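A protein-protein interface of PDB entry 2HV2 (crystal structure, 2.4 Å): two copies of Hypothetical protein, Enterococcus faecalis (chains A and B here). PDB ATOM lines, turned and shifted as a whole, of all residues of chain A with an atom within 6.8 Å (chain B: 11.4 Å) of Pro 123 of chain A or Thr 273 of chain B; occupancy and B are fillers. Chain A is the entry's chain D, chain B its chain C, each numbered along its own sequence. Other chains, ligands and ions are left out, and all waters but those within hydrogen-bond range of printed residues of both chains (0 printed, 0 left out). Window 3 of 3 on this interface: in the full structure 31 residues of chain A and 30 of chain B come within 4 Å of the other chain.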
ATOM      1  N   PRO A 119     -17.437 -34.295   4.902  1.00  0.00           N
ATOM      2  CA  PRO A 119     -16.110 -34.717   4.465  1.00  0.00           C
ATOM      3  C   PRO A 119     -15.142 -35.078   5.592  1.00  0.00           C
ATOM      4  O   PRO A 119     -15.074 -34.368   6.588  1.00  0.00           O
ATOM      5  CB  PRO A 119     -15.610 -33.488   3.692  1.00  0.00           C
ATOM      6  CG  PRO A 119     -16.215 -32.337   4.400  1.00  0.00           C
ATOM      7  CD  PRO A 119     -17.544 -32.823   4.924  1.00  0.00           C
ATOM      8  N   SER A 121     -12.058 -34.939   4.764  1.00  0.00           N
ATOM      9  CA  SER A 121     -11.119 -33.960   4.244  1.00  0.00           C
ATOM     10  C   SER A 121     -11.793 -33.153   3.154  1.00  0.00           C
ATOM     11  O   SER A 121     -12.365 -33.720   2.222  1.00  0.00           O
ATOM     12  CB  SER A 121      -9.893 -34.653   3.648  1.00  0.00           C
ATOM     13  OG  SER A 121      -9.362 -33.881   2.582  1.00  0.00           O
ATOM     14  N   TYR A 122     -11.751 -31.829   3.221  1.00  0.00           N
ATOM     15  CA  TYR A 122     -12.414 -30.947   2.269  1.00  0.00           C
ATOM     16  C   TYR A 122     -11.780 -31.020   0.883  1.00  0.00           C
ATOM     17  O   TYR A 122     -12.515 -31.172  -0.089  1.00  0.00           O
ATOM     18  CB  TYR A 122     -12.467 -29.489   2.818  1.00  0.00           C
ATOM     19  CG  TYR A 122     -13.572 -29.381   3.845  1.00  0.00           C
ATOM     20  CD1 TYR A 122     -13.389 -29.866   5.154  1.00  0.00           C
ATOM     21  CD2 TYR A 122     -14.832 -28.910   3.496  1.00  0.00           C
ATOM     22  CE1 TYR A 122     -14.410 -29.833   6.074  1.00  0.00           C
ATOM     23  CE2 TYR A 122     -15.861 -28.878   4.422  1.00  0.00           C
ATOM     24  CZ  TYR A 122     -15.636 -29.334   5.711  1.00  0.00           C
ATOM     25  OH  TYR A 122     -16.647 -29.316   6.626  1.00  0.00           O
ATOM     26  N   PRO A 123     -10.454 -30.908   0.765  1.00  0.00           N
ATOM     27  CA  PRO A 123      -9.816 -31.038  -0.545  1.00  0.00           C
ATOM     28  C   PRO A 123     -10.099 -32.392  -1.215  1.00  0.00           C
ATOM     29  O   PRO A 123     -10.247 -32.474  -2.443  1.00  0.00           O
ATOM     30  CB  PRO A 123      -8.320 -30.884  -0.231  1.00  0.00           C
ATOM     31  CG  PRO A 123      -8.269 -30.158   1.068  1.00  0.00           C
ATOM     32  CD  PRO A 123      -9.466 -30.620   1.823  1.00  0.00           C
ATOM     33  N   PHE A 124     -10.210 -33.476  -0.472  1.00  0.00           N
ATOM     34  CA  PHE A 124     -10.464 -34.761  -1.060  1.00  0.00           C
ATOM     35  C   PHE A 124     -11.741 -34.730  -1.873  1.00  0.00           C
ATOM     36  O   PHE A 124     -11.753 -35.252  -2.987  1.00  0.00           O
ATOM     37  CB  PHE A 124     -10.538 -35.839   0.023  1.00  0.00           C
ATOM     38  CG  PHE A 124     -10.778 -37.213  -0.508  1.00  0.00           C
ATOM     39  CD1 PHE A 124      -9.741 -37.976  -0.950  1.00  0.00           C
ATOM     40  CD2 PHE A 124     -12.032 -37.732  -0.540  1.00  0.00           C
ATOM     41  CE1 PHE A 124      -9.958 -39.235  -1.426  1.00  0.00           C
ATOM     42  CE2 PHE A 124     -12.261 -38.991  -1.021  1.00  0.00           C
ATOM     43  CZ  PHE A 124     -11.222 -39.740  -1.470  1.00  0.00           C
ATOM     44  N   TYR A 125     -12.842 -34.137  -1.396  1.00  0.00           N
ATOM     45  CA  TYR A 125     -14.120 -34.153  -2.142  1.00  0.00           C
ATOM     46  C   TYR A 125     -14.265 -32.952  -3.059  1.00  0.00           C
ATOM     47  O   TYR A 125     -14.931 -33.018  -4.084  1.00  0.00           O
ATOM     48  CB  TYR A 125     -15.291 -34.209  -1.191  1.00  0.00           C
ATOM     49  CG  TYR A 125     -15.359 -35.489  -0.391  1.00  0.00           C
ATOM     50  CD1 TYR A 125     -14.971 -35.508   0.935  1.00  0.00           C
ATOM     51  CD2 TYR A 125     -15.839 -36.687  -0.962  1.00  0.00           C
ATOM     52  CE1 TYR A 125     -15.050 -36.657   1.687  1.00  0.00           C
ATOM     53  CE2 TYR A 125     -15.907 -37.855  -0.218  1.00  0.00           C
ATOM     54  CZ  TYR A 125     -15.507 -37.831   1.116  1.00  0.00           C
ATOM     55  OH  TYR A 125     -15.567 -38.973   1.894  1.00  0.00           O
ATOM     56  N   ARG A 126     -13.654 -31.819  -2.758  1.00  0.00           N
ATOM     57  CA  ARG A 126     -13.620 -30.706  -3.687  1.00  0.00           C
ATOM     58  C   ARG A 126     -13.093 -31.151  -5.061  1.00  0.00           C
ATOM     59  O   ARG A 126     -13.521 -30.612  -6.073  1.00  0.00           O
ATOM     60  CB  ARG A 126     -12.768 -29.584  -3.118  1.00  0.00           C
ATOM     61  CG  ARG A 126     -12.668 -28.379  -4.036  1.00  0.00           C
ATOM     62  CD  ARG A 126     -11.921 -27.214  -3.428  1.00  0.00           C
ATOM     63  NE  ARG A 126     -12.522 -26.859  -2.143  1.00  0.00           N
ATOM     64  CZ  ARG A 126     -11.953 -27.002  -0.946  1.00  0.00           C
ATOM     65  NH1 ARG A 126     -10.732 -27.483  -0.803  1.00  0.00           N
ATOM     66  NH2 ARG A 126     -12.631 -26.637   0.124  1.00  0.00           N
ATOM     67  N   GLN A 127     -12.195 -32.134  -5.172  1.00  0.00           N
ATOM     68  CA  GLN A 127     -11.718 -32.624  -6.488  1.00  0.00           C
ATOM     69  C   GLN A 127     -12.863 -33.218  -7.327  1.00  0.00           C
ATOM     70  O   GLN A 127     -12.755 -33.308  -8.561  1.00  0.00           O
ATOM     71  CB  GLN A 127     -10.589 -33.660  -6.316  1.00  0.00           C
ATOM     72  CG  GLN A 127     -11.059 -34.966  -5.688  1.00  0.00           C
ATOM     73  CD  GLN A 127      -9.960 -36.017  -5.511  1.00  0.00           C
ATOM     74  OE1 GLN A 127      -9.038 -36.115  -6.328  1.00  0.00           O
ATOM     75  NE2 GLN A 127     -10.091 -36.840  -4.462  1.00  0.00           N
ATOM     76  N   TYR A 128     -13.974 -33.634  -6.720  1.00  0.00           N
ATOM     77  CA  TYR A 128     -15.116 -34.221  -7.424  1.00  0.00           C
ATOM     78  C   TYR A 128     -16.241 -33.206  -7.680  1.00  0.00           C
ATOM     79  O   TYR A 128     -17.265 -33.582  -8.262  1.00  0.00           O
ATOM     80  CB  TYR A 128     -15.673 -35.420  -6.629  1.00  0.00           C
ATOM     81  CG  TYR A 128     -14.643 -36.473  -6.334  1.00  0.00           C
ATOM     82  CD1 TYR A 128     -14.378 -36.894  -5.020  1.00  0.00           C
ATOM     83  CD2 TYR A 128     -13.899 -37.031  -7.365  1.00  0.00           C
ATOM     84  CE1 TYR A 128     -13.401 -37.850  -4.760  1.00  0.00           C
ATOM     85  CE2 TYR A 128     -12.929 -37.987  -7.117  1.00  0.00           C
ATOM     86  CZ  TYR A 128     -12.680 -38.393  -5.818  1.00  0.00           C
ATOM     87  OH  TYR A 128     -11.710 -39.337  -5.592  1.00  0.00           O
ATOM     88  N   GLN A 132     -17.836 -26.585   0.501  1.00  0.00           N
ATOM     89  CA  GLN A 132     -18.488 -26.230   1.709  1.00  0.00           C
ATOM     90  C   GLN A 132     -19.621 -25.297   1.360  1.00  0.00           C
ATOM     91  O   GLN A 132     -19.419 -24.314   0.649  1.00  0.00           O
ATOM     92  CB  GLN A 132     -17.512 -25.556   2.665  1.00  0.00           C
ATOM     93  CG  GLN A 132     -18.061 -25.396   4.070  1.00  0.00           C
ATOM     94  CD  GLN A 132     -17.074 -24.739   5.009  1.00  0.00           C
ATOM     95  OE1 GLN A 132     -17.475 -24.185   6.045  1.00  0.00           O
ATOM     96  NE2 GLN A 132     -15.784 -24.783   4.658  1.00  0.00           N
ATOM     97  N   MET A 285     -20.496 -30.397   2.655  1.00  0.00           N
ATOM     98  CA  MET A 285     -20.224 -29.850   1.352  1.00  0.00           C
ATOM     99  C   MET A 285     -21.375 -30.185   0.449  1.00  0.00           C
ATOM    100  O   MET A 285     -22.116 -31.120   0.705  1.00  0.00           O
ATOM    101  CB  MET A 285     -18.950 -30.455   0.759  1.00  0.00           C
ATOM    102  CG  MET A 285     -17.706 -30.196   1.582  1.00  0.00           C
ATOM    103  SD  MET A 285     -16.118 -31.103   0.893  1.00  0.00           S
ATOM    104  CE  MET A 285     -15.373 -29.654  -0.194  1.00  0.00           C
ATOM    105  N   TYR B 139     -10.219 -15.947  15.410  1.00  0.00           N
ATOM    106  CA  TYR B 139      -9.617 -17.043  14.663  1.00  0.00           C
ATOM    107  C   TYR B 139      -8.300 -17.488  15.269  1.00  0.00           C
ATOM    108  O   TYR B 139      -7.483 -16.655  15.635  1.00  0.00           O
ATOM    109  CB  TYR B 139      -9.318 -16.630  13.237  1.00  0.00           C
ATOM    110  CG  TYR B 139     -10.485 -16.151  12.460  1.00  0.00           C
ATOM    111  CD1 TYR B 139     -10.944 -14.852  12.603  1.00  0.00           C
ATOM    112  CD2 TYR B 139     -11.096 -16.967  11.527  1.00  0.00           C
ATOM    113  CE1 TYR B 139     -12.031 -14.398  11.893  1.00  0.00           C
ATOM    114  CE2 TYR B 139     -12.168 -16.512  10.777  1.00  0.00           C
ATOM    115  CZ  TYR B 139     -12.630 -15.229  10.973  1.00  0.00           C
ATOM    116  OH  TYR B 139     -13.679 -14.762  10.237  1.00  0.00           O
ATOM    117  N   THR B 140      -8.040 -18.787  15.378  1.00  0.00           N
ATOM    118  CA  THR B 140      -6.776 -19.326  15.903  1.00  0.00           C
ATOM    119  C   THR B 140      -6.409 -20.454  14.992  1.00  0.00           C
ATOM    120  O   THR B 140      -7.204 -21.364  14.821  1.00  0.00           O
ATOM    121  CB  THR B 140      -6.954 -19.832  17.340  1.00  0.00           C
ATOM    122  OG1 THR B 140      -7.552 -18.790  18.109  1.00  0.00           O
ATOM    123  CG2 THR B 140      -5.631 -20.242  17.969  1.00  0.00           C
ATOM    124  N   ILE B 141      -5.277 -20.424  14.306  1.00  0.00           N
ATOM    125  CA  ILE B 141      -4.920 -21.483  13.377  1.00  0.00           C
ATOM    126  C   ILE B 141      -3.493 -21.947  13.659  1.00  0.00           C
ATOM    127  O   ILE B 141      -2.591 -21.139  13.876  1.00  0.00           O
ATOM    128  CB  ILE B 141      -5.130 -21.025  11.904  1.00  0.00           C
ATOM    129  CG1 ILE B 141      -4.840 -22.173  10.938  1.00  0.00           C
ATOM    130  CG2 ILE B 141      -4.261 -19.849  11.556  1.00  0.00           C
ATOM    131  CD1 ILE B 141      -5.598 -22.065   9.631  1.00  0.00           C
ATOM    132  N   LYS B 142      -3.239 -23.248  13.700  1.00  0.00           N
ATOM    133  CA  LYS B 142      -1.905 -23.783  13.947  1.00  0.00           C
ATOM    134  C   LYS B 142      -0.967 -23.420  12.806  1.00  0.00           C
ATOM    135  O   LYS B 142      -1.395 -23.285  11.638  1.00  0.00           O
ATOM    136  CB  LYS B 142      -1.967 -25.300  14.096  1.00  0.00           C
ATOM    137  CG  LYS B 142      -2.782 -25.779  15.287  1.00  0.00           C
ATOM    138  CD  LYS B 142      -2.949 -27.294  15.288  1.00  0.00           C
ATOM    139  CE  LYS B 142      -3.975 -27.755  16.313  1.00  0.00           C
ATOM    140  NZ  LYS B 142      -5.384 -27.580  15.848  1.00  0.00           N
ATOM    141  N   THR B 143       0.330 -23.276  13.078  1.00  0.00           N
ATOM    142  CA  THR B 143       1.306 -22.834  12.088  1.00  0.00           C
ATOM    143  C   THR B 143       1.315 -23.760  10.855  1.00  0.00           C
ATOM    144  O   THR B 143       1.409 -23.284   9.713  1.00  0.00           O
ATOM    145  CB  THR B 143       2.701 -22.729  12.732  1.00  0.00           C
ATOM    146  OG1 THR B 143       3.582 -22.039  11.854  1.00  0.00           O
ATOM    147  CG2 THR B 143       3.286 -24.094  13.039  1.00  0.00           C
ATOM    148  N   GLU B 144       1.162 -25.073  11.007  1.00  0.00           N
ATOM    149  CA  GLU B 144       1.179 -26.017   9.866  1.00  0.00           C
ATOM    150  C   GLU B 144      -0.055 -25.863   8.998  1.00  0.00           C
ATOM    151  O   GLU B 144      -0.090 -26.351   7.876  1.00  0.00           O
ATOM    152  CB  GLU B 144       1.176 -27.474  10.337  1.00  0.00           C
ATOM    153  CG  GLU B 144       1.803 -27.719  11.710  1.00  0.00           C
ATOM    154  CD  GLU B 144       0.846 -27.475  12.869  1.00  0.00           C
ATOM    155  OE1 GLU B 144      -0.218 -28.132  12.901  1.00  0.00           O
ATOM    156  OE2 GLU B 144       1.181 -26.636  13.753  1.00  0.00           O
ATOM    157  N   ASP B 145      -1.115 -25.233   9.497  1.00  0.00           N
ATOM    158  CA  ASP B 145      -2.397 -25.162   8.850  1.00  0.00           C
ATOM    159  C   ASP B 145      -2.533 -23.870   8.073  1.00  0.00           C
ATOM    160  O   ASP B 145      -3.466 -23.717   7.267  1.00  0.00           O
ATOM    161  CB  ASP B 145      -3.493 -25.268   9.922  1.00  0.00           C
ATOM    162  CG  ASP B 145      -3.641 -26.676  10.466  1.00  0.00           C
ATOM    163  OD1 ASP B 145      -3.193 -27.621   9.776  1.00  0.00           O
ATOM    164  OD2 ASP B 145      -4.217 -26.938  11.547  1.00  0.00           O
ATOM    165  N   TRP B 146      -1.642 -22.901   8.276  1.00  0.00           N
ATOM    166  CA  TRP B 146      -1.663 -21.680   7.521  1.00  0.00           C
ATOM    167  C   TRP B 146      -1.368 -22.073   6.067  1.00  0.00           C
ATOM    168  O   TRP B 146      -0.367 -22.735   5.808  1.00  0.00           O
ATOM    169  CB  TRP B 146      -0.660 -20.635   8.055  1.00  0.00           C
ATOM    170  CG  TRP B 146      -0.890 -19.339   7.351  1.00  0.00           C
ATOM    171  CD1 TRP B 146      -0.450 -19.008   6.113  1.00  0.00           C
ATOM    172  CD2 TRP B 146      -1.707 -18.255   7.789  1.00  0.00           C
ATOM    173  NE1 TRP B 146      -0.924 -17.773   5.760  1.00  0.00           N
ATOM    174  CE2 TRP B 146      -1.701 -17.291   6.775  1.00  0.00           C
ATOM    175  CE3 TRP B 146      -2.439 -17.993   8.954  1.00  0.00           C
ATOM    176  CZ2 TRP B 146      -2.397 -16.095   6.875  1.00  0.00           C
ATOM    177  CZ3 TRP B 146      -3.118 -16.800   9.053  1.00  0.00           C
ATOM    178  CH2 TRP B 146      -3.091 -15.865   8.022  1.00  0.00           C
ATOM    179  N   PRO B 147      -2.241 -21.687   5.129  1.00  0.00           N
ATOM    180  CA  PRO B 147      -2.141 -22.176   3.754  1.00  0.00           C
ATOM    181  C   PRO B 147      -0.990 -21.563   2.967  1.00  0.00           C
ATOM    182  O   PRO B 147      -0.673 -20.381   3.130  1.00  0.00           O
ATOM    183  CB  PRO B 147      -3.476 -21.750   3.134  1.00  0.00           C
ATOM    184  CG  PRO B 147      -3.842 -20.524   3.878  1.00  0.00           C
ATOM    185  CD  PRO B 147      -3.370 -20.745   5.280  1.00  0.00           C
ATOM    186  N   ARG B 148      -0.335 -22.324   2.106  1.00  0.00           N
ATOM    187  CA  ARG B 148       0.624 -21.794   1.167  1.00  0.00           C
ATOM    188  C   ARG B 148      -0.146 -20.957   0.146  1.00  0.00           C
ATOM    189  O   ARG B 148      -1.238 -21.330  -0.278  1.00  0.00           O
ATOM    190  CB  ARG B 148       1.418 -22.926   0.479  1.00  0.00           C
ATOM    191  CG  ARG B 148       2.123 -23.896   1.444  1.00  0.00           C
ATOM    192  CD  ARG B 148       3.609 -24.134   1.137  1.00  0.00           C
ATOM    193  NE  ARG B 148       3.868 -24.856  -0.126  1.00  0.00           N
ATOM    194  CZ  ARG B 148       5.029 -24.812  -0.820  1.00  0.00           C
ATOM    195  NH1 ARG B 148       6.067 -24.069  -0.408  1.00  0.00           N
ATOM    196  NH2 ARG B 148       5.152 -25.509  -1.954  1.00  0.00           N
ATOM    197  N   VAL B 149       0.376 -19.800  -0.251  1.00  0.00           N
ATOM    198  CA  VAL B 149      -0.311 -18.851  -1.114  1.00  0.00           C
ATOM    199  C   VAL B 149       0.672 -18.501  -2.210  1.00  0.00           C
ATOM    200  O   VAL B 149       1.778 -18.078  -1.908  1.00  0.00           O
ATOM    201  CB  VAL B 149      -0.699 -17.559  -0.361  1.00  0.00           C
ATOM    202  CG1 VAL B 149      -1.724 -16.773  -1.156  1.00  0.00           C
ATOM    203  CG2 VAL B 149      -1.224 -17.871   1.035  1.00  0.00           C
ATOM    204  N   ASP B 266     -17.756 -16.105   8.530  1.00  0.00           N
ATOM    205  CA  ASP B 266     -16.333 -16.190   8.873  1.00  0.00           C
ATOM    206  C   ASP B 266     -15.490 -16.496   7.652  1.00  0.00           C
ATOM    207  O   ASP B 266     -16.005 -16.864   6.596  1.00  0.00           O
ATOM    208  CB  ASP B 266     -16.081 -17.226   9.979  1.00  0.00           C
ATOM    209  CG  ASP B 266     -16.266 -18.653   9.525  1.00  0.00           C
ATOM    210  OD1 ASP B 266     -16.616 -19.487  10.385  1.00  0.00           O
ATOM    211  OD2 ASP B 266     -16.070 -19.060   8.354  1.00  0.00           O
ATOM    212  N   LEU B 267     -14.178 -16.353   7.764  1.00  0.00           N
ATOM    213  CA  LEU B 267     -13.247 -16.476   6.664  1.00  0.00           C
ATOM    214  C   LEU B 267     -12.774 -17.923   6.519  1.00  0.00           C
ATOM    215  O   LEU B 267     -12.058 -18.255   5.581  1.00  0.00           O
ATOM    216  CB  LEU B 267     -12.058 -15.546   6.922  1.00  0.00           C
ATOM    217  CG  LEU B 267     -12.264 -14.025   6.715  1.00  0.00           C
ATOM    218  CD1 LEU B 267     -13.742 -13.599   6.755  1.00  0.00           C
ATOM    219  CD2 LEU B 267     -11.453 -13.236   7.749  1.00  0.00           C
ATOM    220  N   ASN B 268     -13.163 -18.844   7.393  1.00  0.00           N
ATOM    221  CA  ASN B 268     -12.551 -20.164   7.439  1.00  0.00           C
ATOM    222  C   ASN B 268     -12.660 -20.843   6.100  1.00  0.00           C
ATOM    223  O   ASN B 268     -11.793 -21.607   5.744  1.00  0.00           O
ATOM    224  CB  ASN B 268     -13.195 -21.031   8.522  1.00  0.00           C
ATOM    225  CG  ASN B 268     -12.245 -22.057   9.109  1.00  0.00           C
ATOM    226  OD1 ASN B 268     -11.029 -22.051   8.849  1.00  0.00           O
ATOM    227  ND2 ASN B 268     -12.794 -22.946   9.927  1.00  0.00           N
ATOM    228  N   ASP B 269     -13.672 -20.585   5.284  1.00  0.00           N
ATOM    229  CA  ASP B 269     -13.875 -21.317   4.018  1.00  0.00           C
ATOM    230  C   ASP B 269     -13.021 -20.751   2.885  1.00  0.00           C
ATOM    231  O   ASP B 269     -12.846 -21.401   1.842  1.00  0.00           O
ATOM    232  CB  ASP B 269     -15.339 -21.273   3.620  1.00  0.00           C
ATOM    233  CG  ASP B 269     -15.800 -19.871   3.336  1.00  0.00           C
ATOM    234  OD1 ASP B 269     -16.260 -19.628   2.198  1.00  0.00           O
ATOM    235  OD2 ASP B 269     -15.707 -18.942   4.181  1.00  0.00           O
ATOM    236  N   LEU B 270     -12.449 -19.558   3.017  1.00  0.00           N
ATOM    237  CA  LEU B 270     -11.475 -19.054   2.052  1.00  0.00           C
ATOM    238  C   LEU B 270     -10.185 -19.898   2.018  1.00  0.00           C
ATOM    239  O   LEU B 270      -9.309 -19.662   1.185  1.00  0.00           O
ATOM    240  CB  LEU B 270     -11.149 -17.599   2.368  1.00  0.00           C
ATOM    241  CG  LEU B 270     -12.343 -16.642   2.268  1.00  0.00           C
ATOM    242  CD1 LEU B 270     -11.893 -15.203   2.470  1.00  0.00           C
ATOM    243  CD2 LEU B 270     -13.071 -16.801   0.920  1.00  0.00           C
ATOM    244  N   MET B 271     -10.002 -20.888   2.889  1.00  0.00           N
ATOM    245  CA  MET B 271      -8.914 -21.842   2.798  1.00  0.00           C
ATOM    246  C   MET B 271      -9.406 -23.154   2.179  1.00  0.00           C
ATOM    247  O   MET B 271     -10.581 -23.493   2.309  1.00  0.00           O
ATOM    248  CB  MET B 271      -8.379 -22.121   4.194  1.00  0.00           C
ATOM    249  CG  MET B 271      -7.646 -20.947   4.800  1.00  0.00           C
ATOM    250  SD  MET B 271      -7.217 -21.255   6.681  1.00  0.00           S
ATOM    251  CE  MET B 271      -8.946 -20.795   7.472  1.00  0.00           C
ATOM    252  N   PRO B 272      -8.519 -23.892   1.517  1.00  0.00           N
ATOM    253  CA  PRO B 272      -8.841 -25.243   1.054  1.00  0.00           C
ATOM    254  C   PRO B 272      -9.178 -26.183   2.210  1.00  0.00           C
ATOM    255  O   PRO B 272      -9.996 -27.102   2.049  1.00  0.00           O
ATOM    256  CB  PRO B 272      -7.547 -25.711   0.352  1.00  0.00           C
ATOM    257  CG  PRO B 272      -6.740 -24.484   0.103  1.00  0.00           C
ATOM    258  CD  PRO B 272      -7.148 -23.485   1.143  1.00  0.00           C
ATOM    259  N   THR B 273      -8.543 -26.032   3.374  1.00  0.00           N
ATOM    260  CA  THR B 273      -8.910 -26.746   4.589  1.00  0.00           C
ATOM    261  C   THR B 273      -9.361 -25.703   5.613  1.00  0.00           C
ATOM    262  O   THR B 273      -8.575 -24.856   6.038  1.00  0.00           O
ATOM    263  CB  THR B 273      -7.729 -27.570   5.126  1.00  0.00           C
ATOM    264  OG1 THR B 273      -7.252 -28.453   4.098  1.00  0.00           O
ATOM    265  CG2 THR B 273      -8.154 -28.378   6.341  1.00  0.00           C
ATOM    266  N   PRO B 274     -10.633 -25.739   5.991  1.00  0.00           N
ATOM    267  CA  PRO B 274     -11.150 -24.774   6.935  1.00  0.00           C
ATOM    268  C   PRO B 274     -10.646 -25.128   8.342  1.00  0.00           C
ATOM    269  O   PRO B 274     -11.419 -25.496   9.232  1.00  0.00           O
ATOM    270  CB  PRO B 274     -12.655 -24.909   6.760  1.00  0.00           C
ATOM    271  CG  PRO B 274     -12.853 -26.334   6.371  1.00  0.00           C
ATOM    272  CD  PRO B 274     -11.655 -26.717   5.579  1.00  0.00           C
ATOM    273  N   ALA B 275      -9.347 -25.010   8.580  1.00  0.00           N
ATOM    274  CA  ALA B 275      -8.680 -25.493   9.763  1.00  0.00           C
ATOM    275  C   ALA B 275      -8.617 -24.423  10.876  1.00  0.00           C
ATOM    276  O   ALA B 275      -8.041 -24.682  11.928  1.00  0.00           O
ATOM    277  CB  ALA B 275      -7.264 -25.950   9.363  1.00  0.00           C
ATOM    278  N   ALA B 276      -9.158 -23.212  10.713  1.00  0.00           N
ATOM    279  CA  ALA B 276      -9.143 -22.209  11.778  1.00  0.00           C
ATOM    280  C   ALA B 276     -10.181 -22.587  12.799  1.00  0.00           C
ATOM    281  O   ALA B 276     -11.298 -23.000  12.458  1.00  0.00           O
ATOM    282  CB  ALA B 276      -9.415 -20.791  11.260  1.00  0.00           C
ATOM    283  N   SER B 277      -9.851 -22.515  14.078  1.00  0.00           N
ATOM    284  CA  SER B 277     -10.827 -22.534  15.132  1.00  0.00           C
ATOM    285  C   SER B 277     -11.491 -21.153  15.129  1.00  0.00           C
ATOM    286  O   SER B 277     -10.791 -20.138  15.231  1.00  0.00           O
ATOM    287  CB  SER B 277     -10.124 -22.829  16.450  1.00  0.00           C
ATOM    288  OG  SER B 277     -10.986 -22.558  17.525  1.00  0.00           O
ATOM    289  N   VAL B 278     -12.819 -21.049  14.978  1.00  0.00           N
ATOM    290  CA  VAL B 278     -13.562 -19.766  14.937  1.00  0.00           C
ATOM    291  C   VAL B 278     -14.553 -19.647  16.103  1.00  0.00           C
ATOM    292  O   VAL B 278     -15.471 -20.431  16.224  1.00  0.00           O
ATOM    293  CB  VAL B 278     -14.359 -19.588  13.624  1.00  0.00           C
ATOM    294  CG1 VAL B 278     -15.084 -18.246  13.607  1.00  0.00           C
ATOM    295  CG2 VAL B 278     -13.455 -19.718  12.412  1.00  0.00           C
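The backbone carbonyl oxygen (O) of Pro 272 of chain B sits at hydrogen-bond distance from the guanidinium group (NH1) of Arg 126 of chain A, 3.0 Å away.
The backbone carbonyl oxygen of Pro 274 of chain B is in hydrogen-bond range of the side-chain amide nitrogen of Asn 268 of chain B (3.0 Å).
Among the printed residues, pairs that only touch across the chains: Tyr 122 of chain A with Pro 272 of chain B (3.5 Å), Tyr 122 of chain A with Pro 274 of chain B (3.6 Å), Pro 123 of chain A with Pro 272 of chain B (3.6 Å), Pro 123 of chain A with Thr 273 of chain B (3.6 Å), Gln 132 of chain A with Asp 269 of chain B (3.7 Å) and Gln 132 of chain A with Pro 274 of chain B (3.7 Å).
Of the printed residues of chain B, Pro 123 of chain A touches Pro 272 (3.6 Å) and Thr 273 (3.6 Å). Of chain B, only Pro 272 comes within 4 Å of Arg 126 of chain A. Of the printed residues of chain B, Gln 132 of chain A touches Asp 269 (3.7 Å) and Pro 274 (3.7 Å). Of the printed residues of chain A, Pro 274 of chain B touches Tyr 122 (3.6 Å) and Gln 132 (3.7 Å). Of the printed residues of chain A, Pro 272 of chain B touches Tyr 122, Pro 123 and Arg 126. Of the printed residues of chain B, Tyr 122 of chain A touches Pro 272 and Pro 274. Printed residues of chain A within 4 Å of Asp 269 of chain B: Gln 132 (3.7 Å). The nearest printed residue of chain A that does not touch Pro 274 of chain B is Arg 126 of chain A (5.5 Å).
Of the 11 printed residues of chain A, 4 touch a printed residue of chain B. Printed residues of chain B that touch a printed residue of chain A: Asp 269, Pro 272, Thr 273 and Pro 274. Among the printed residues, no Asp or Glu carboxylate lies within 4 Å of a Lys or Arg side-chain nitrogen of the other chain.
No position is printed for both chains. Of the 7 pairs that touch across the chains among the printed residues, none has its exchanged pair printed and touching as well.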
